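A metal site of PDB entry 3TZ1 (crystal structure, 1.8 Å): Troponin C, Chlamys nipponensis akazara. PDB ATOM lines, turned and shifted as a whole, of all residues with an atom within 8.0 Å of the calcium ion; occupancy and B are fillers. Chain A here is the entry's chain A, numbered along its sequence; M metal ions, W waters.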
ATOM      1  N   VAL A  23       5.169 -21.250 -15.533  1.00  0.00           N
ATOM      2  CA  VAL A  23       6.603 -21.306 -15.223  1.00  0.00           C
ATOM      3  C   VAL A  23       6.823 -21.870 -13.825  1.00  0.00           C
ATOM      4  O   VAL A  23       5.897 -21.951 -13.029  1.00  0.00           O
ATOM      5  CB  VAL A  23       7.270 -19.912 -15.274  1.00  0.00           C
ATOM      6  CG1 VAL A  23       7.259 -19.353 -16.692  1.00  0.00           C
ATOM      7  CG2 VAL A  23       6.598 -18.952 -14.292  1.00  0.00           C
ATOM      8  N   ILE A  24       8.056 -22.276 -13.547  1.00  0.00           N
ATOM      9  CA  ILE A  24       8.458 -22.611 -12.195  1.00  0.00           C
ATOM     10  C   ILE A  24       9.353 -21.467 -11.699  1.00  0.00           C
ATOM     11  O   ILE A  24      10.359 -21.177 -12.317  1.00  0.00           O
ATOM     12  CB  ILE A  24       9.244 -23.937 -12.172  1.00  0.00           C
ATOM     13  CG1 ILE A  24       8.408 -25.057 -12.791  1.00  0.00           C
ATOM     14  CG2 ILE A  24       9.644 -24.301 -10.733  1.00  0.00           C
ATOM     15  CD1 ILE A  24       9.174 -26.347 -13.027  1.00  0.00           C
ATOM     16  N   VAL A  26      12.165 -19.596  -9.620  1.00  0.00           N
ATOM     17  CA  VAL A  26      13.463 -20.103  -9.179  1.00  0.00           C
ATOM     18  C   VAL A  26      13.482 -20.367  -7.662  1.00  0.00           C
ATOM     19  O   VAL A  26      14.246 -21.210  -7.197  1.00  0.00           O
ATOM     20  CB  VAL A  26      14.604 -19.166  -9.648  1.00  0.00           C
ATOM     21  CG1 VAL A  26      15.760 -19.196  -8.664  1.00  0.00           C
ATOM     22  CG2 VAL A  26      15.039 -19.566 -11.049  1.00  0.00           C
ATOM     23  N   ILE A  49      20.810 -23.514 -10.214  1.00  0.00           N
ATOM     24  CA  ILE A  49      19.734 -22.633 -10.660  1.00  0.00           C
ATOM     25  C   ILE A  49      20.039 -22.024 -12.028  1.00  0.00           C
ATOM     26  O   ILE A  49      19.223 -22.056 -12.947  1.00  0.00           O
ATOM     27  CB  ILE A  49      19.471 -21.512  -9.635  1.00  0.00           C
ATOM     28  CG1 ILE A  49      18.840 -22.097  -8.361  1.00  0.00           C
ATOM     29  CG2 ILE A  49      18.541 -20.472 -10.232  1.00  0.00           C
ATOM     30  CD1 ILE A  49      18.632 -21.064  -7.274  1.00  0.00           C
ATOM     31  N   THR A  52      19.641 -24.214 -14.967  1.00  0.00           N
ATOM     32  CA  THR A  52      18.247 -24.490 -15.284  1.00  0.00           C
ATOM     33  C   THR A  52      17.583 -23.290 -15.947  1.00  0.00           C
ATOM     34  O   THR A  52      17.001 -23.397 -17.037  1.00  0.00           O
ATOM     35  CB  THR A  52      17.435 -24.906 -14.059  1.00  0.00           C
ATOM     36  OG1 THR A  52      18.152 -25.890 -13.313  1.00  0.00           O
ATOM     37  CG2 THR A  52      16.098 -25.491 -14.494  1.00  0.00           C
ATOM     38  N   ASP A  53      17.613 -22.165 -15.250  1.00  0.00           N
ATOM     39  CA  ASP A  53      17.003 -20.955 -15.761  1.00  0.00           C
ATOM     40  C   ASP A  53      18.105 -20.283 -16.562  1.00  0.00           C
ATOM     41  O   ASP A  53      18.941 -19.530 -16.034  1.00  0.00           O
ATOM     42  CB  ASP A  53      16.599 -20.102 -14.557  1.00  0.00           C
ATOM     43  CG  ASP A  53      16.224 -18.685 -14.929  1.00  0.00           C
ATOM     44  OD1 ASP A  53      15.785 -18.494 -16.071  1.00  0.00           O
ATOM     45  OD2 ASP A  53      16.362 -17.764 -14.084  1.00  0.00           O
ATOM     46  N   THR A  54      18.054 -20.483 -17.862  1.00  0.00           N
ATOM     47  CA  THR A  54      19.218 -20.161 -18.691  1.00  0.00           C
ATOM     48  C   THR A  54      19.236 -18.705 -19.151  1.00  0.00           C
ATOM     49  O   THR A  54      20.284 -18.171 -19.539  1.00  0.00           O
ATOM     50  CB  THR A  54      19.355 -21.139 -19.885  1.00  0.00           C
ATOM     51  OG1 THR A  54      18.093 -21.279 -20.533  1.00  0.00           O
ATOM     52  CG2 THR A  54      19.804 -22.513 -19.393  1.00  0.00           C
ATOM     53  N   ASP A  55      18.082 -18.046 -19.089  1.00  0.00           N
ATOM     54  CA  ASP A  55      18.041 -16.635 -19.450  1.00  0.00           C
ATOM     55  C   ASP A  55      18.091 -15.677 -18.258  1.00  0.00           C
ATOM     56  O   ASP A  55      18.037 -14.466 -18.427  1.00  0.00           O
ATOM     57  CB  ASP A  55      16.885 -16.317 -20.423  1.00  0.00           C
ATOM     58  CG  ASP A  55      15.540 -16.764 -19.898  1.00  0.00           C
ATOM     59  OD1 ASP A  55      15.428 -16.972 -18.681  1.00  0.00           O
ATOM     60  OD2 ASP A  55      14.594 -16.907 -20.701  1.00  0.00           O
ATOM     61  N   GLY A  56      18.215 -16.241 -17.058  1.00  0.00           N
ATOM     62  CA  GLY A  56      18.275 -15.438 -15.840  1.00  0.00           C
ATOM     63  C   GLY A  56      17.010 -14.640 -15.605  1.00  0.00           C
ATOM     64  O   GLY A  56      17.048 -13.539 -15.062  1.00  0.00           O
ATOM     65  N   SER A  57      15.871 -15.187 -16.017  1.00  0.00           N
ATOM     66  CA  SER A  57      14.604 -14.474 -15.875  1.00  0.00           C
ATOM     67  C   SER A  57      14.019 -14.665 -14.484  1.00  0.00           C
ATOM     68  O   SER A  57      13.068 -13.977 -14.092  1.00  0.00           O
ATOM     69  CB  SER A  57      13.610 -14.920 -16.948  1.00  0.00           C
ATOM     70  OG  SER A  57      13.085 -16.214 -16.660  1.00  0.00           O
ATOM     71  N   GLY A  58      14.587 -15.604 -13.731  1.00  0.00           N
ATOM     72  CA  GLY A  58      14.085 -15.939 -12.412  1.00  0.00           C
ATOM     73  C   GLY A  58      12.899 -16.874 -12.484  1.00  0.00           C
ATOM     74  O   GLY A  58      12.228 -17.135 -11.485  1.00  0.00           O
ATOM     75  N   THR A  59      12.628 -17.388 -13.685  1.00  0.00           N
ATOM     76  CA  THR A  59      11.535 -18.331 -13.877  1.00  0.00           C
ATOM     77  C   THR A  59      12.004 -19.426 -14.840  1.00  0.00           C
ATOM     78  O   THR A  59      12.777 -19.149 -15.763  1.00  0.00           O
ATOM     79  CB  THR A  59      10.315 -17.642 -14.506  1.00  0.00           C
ATOM     80  OG1 THR A  59      10.721 -17.003 -15.726  1.00  0.00           O
ATOM     81  CG2 THR A  59       9.746 -16.606 -13.567  1.00  0.00           C
ATOM     82  N   VAL A  60      11.540 -20.642 -14.646  1.00  0.00           N
ATOM     83  CA  VAL A  60      11.895 -21.724 -15.539  1.00  0.00           C
ATOM     84  C   VAL A  60      10.719 -22.025 -16.446  1.00  0.00           C
ATOM     85  O   VAL A  60       9.691 -22.500 -15.976  1.00  0.00           O
ATOM     86  CB  VAL A  60      12.275 -22.998 -14.741  1.00  0.00           C
ATOM     87  CG1 VAL A  60      12.613 -24.146 -15.684  1.00  0.00           C
ATOM     88  CG2 VAL A  60      13.470 -22.711 -13.827  1.00  0.00           C
ATOM     89  N   ASP A  61      10.826 -21.726 -17.738  1.00  0.00           N
ATOM     90  CA  ASP A  61       9.715 -22.044 -18.640  1.00  0.00           C
ATOM     91  C   ASP A  61       9.781 -23.514 -19.055  1.00  0.00           C
ATOM     92  O   ASP A  61      10.732 -24.221 -18.712  1.00  0.00           O
ATOM     93  CB  ASP A  61       9.634 -21.074 -19.841  1.00  0.00           C
ATOM     94  CG  ASP A  61      10.894 -21.060 -20.683  1.00  0.00           C
ATOM     95  OD1 ASP A  61      11.352 -22.147 -21.094  1.00  0.00           O
ATOM     96  OD2 ASP A  61      11.420 -19.957 -20.946  1.00  0.00           O
ATOM     97  N   TYR A  62       8.780 -23.990 -19.786  1.00  0.00           N
ATOM     98  CA  TYR A  62       8.717 -25.431 -20.063  1.00  0.00           C
ATOM     99  C   TYR A  62       9.867 -25.881 -20.960  1.00  0.00           C
ATOM    100  O   TYR A  62      10.380 -26.988 -20.819  1.00  0.00           O
ATOM    101  CB  TYR A  62       7.373 -25.838 -20.677  1.00  0.00           C
ATOM    102  CG  TYR A  62       7.280 -27.326 -20.962  1.00  0.00           C
ATOM    103  CD1 TYR A  62       7.335 -27.809 -22.255  1.00  0.00           C
ATOM    104  CD2 TYR A  62       7.144 -28.240 -19.925  1.00  0.00           C
ATOM    105  CE1 TYR A  62       7.259 -29.166 -22.518  1.00  0.00           C
ATOM    106  CE2 TYR A  62       7.072 -29.601 -20.180  1.00  0.00           C
ATOM    107  CZ  TYR A  62       7.116 -30.059 -21.479  1.00  0.00           C
ATOM    108  OH  TYR A  62       7.042 -31.404 -21.723  1.00  0.00           O
ATOM    109  N   GLU A  64      12.896 -24.635 -20.995  1.00  0.00           N
ATOM    110  CA  GLU A  64      14.076 -24.729 -20.134  1.00  0.00           C
ATOM    111  C   GLU A  64      14.001 -25.985 -19.297  1.00  0.00           C
ATOM    112  O   GLU A  64      15.001 -26.673 -19.073  1.00  0.00           O
ATOM    113  CB  GLU A  64      14.191 -23.505 -19.230  1.00  0.00           C
ATOM    114  CG  GLU A  64      14.474 -22.222 -19.968  1.00  0.00           C
ATOM    115  CD  GLU A  64      14.431 -21.030 -19.068  1.00  0.00           C
ATOM    116  OE1 GLU A  64      13.587 -21.022 -18.146  1.00  0.00           O
ATOM    117  OE2 GLU A  64      15.265 -20.114 -19.261  1.00  0.00           O
ATOM    118  N   PHE A  65      12.799 -26.294 -18.830  1.00  0.00           N
ATOM    119  CA  PHE A  65      12.591 -27.456 -17.984  1.00  0.00           C
ATOM    120  C   PHE A  65      12.898 -28.723 -18.795  1.00  0.00           C
ATOM    121  O   PHE A  65      13.573 -29.632 -18.300  1.00  0.00           O
ATOM    122  CB  PHE A  65      11.149 -27.469 -17.479  1.00  0.00           C
ATOM    123  CG  PHE A  65      10.879 -28.494 -16.425  1.00  0.00           C
ATOM    124  CD1 PHE A  65      11.566 -28.465 -15.220  1.00  0.00           C
ATOM    125  CD2 PHE A  65       9.928 -29.495 -16.626  1.00  0.00           C
ATOM    126  CE1 PHE A  65      11.315 -29.417 -14.226  1.00  0.00           C
ATOM    127  CE2 PHE A  65       9.683 -30.447 -15.648  1.00  0.00           C
ATOM    128  CZ  PHE A  65      10.373 -30.402 -14.449  1.00  0.00           C
HETATM  129 CA    CA M   1      14.047 -18.522 -17.640  1.00  0.00          CA
HETATM  130  O   HOH W   1      12.060 -18.206 -19.331  1.00  0.00           O
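The side-chain carboxylate of Asp 61 sits at hydrogen-bond distance from the backbone NH of Glu 64 (2.9 Å). The side-chain carboxylate (OE2) of Glu 64 lies close to the backbone NH (N) of Thr 54 (3.1 Å). The side-chain carboxylate of Asp 53 sits close to the backbone NH of Gly 56 (3.5 Å). OD2 of Asp 53 sits at hydrogen-bond distance from N of Gly 58 (2.8 Å).
The calcium ion is bound by OD1 of Asp 55 (2.3 Å), OD1 of Asp 53 (2.3 Å), O of Thr 59 (2.4 Å), OE2 of Glu 64 (2.6 Å), OE1 of Glu 64 (2.6 Å), water W1 (2.6 Å) and OG of Ser 57 (2.7 Å). The calcium ion has seven donor atoms within binding distance.
Water W1 bridges OD2 of Asp 61 (2.5 Å) and OD2 of Asp 55 (3.2 Å).
Five residues have an atom within 4 Å of the calcium ion: Asp 53, Asp 55, Ser 57, Thr 59 and Glu 64. The nearest printed residue that does not touch the calcium ion is Val 60 (4.4 Å).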
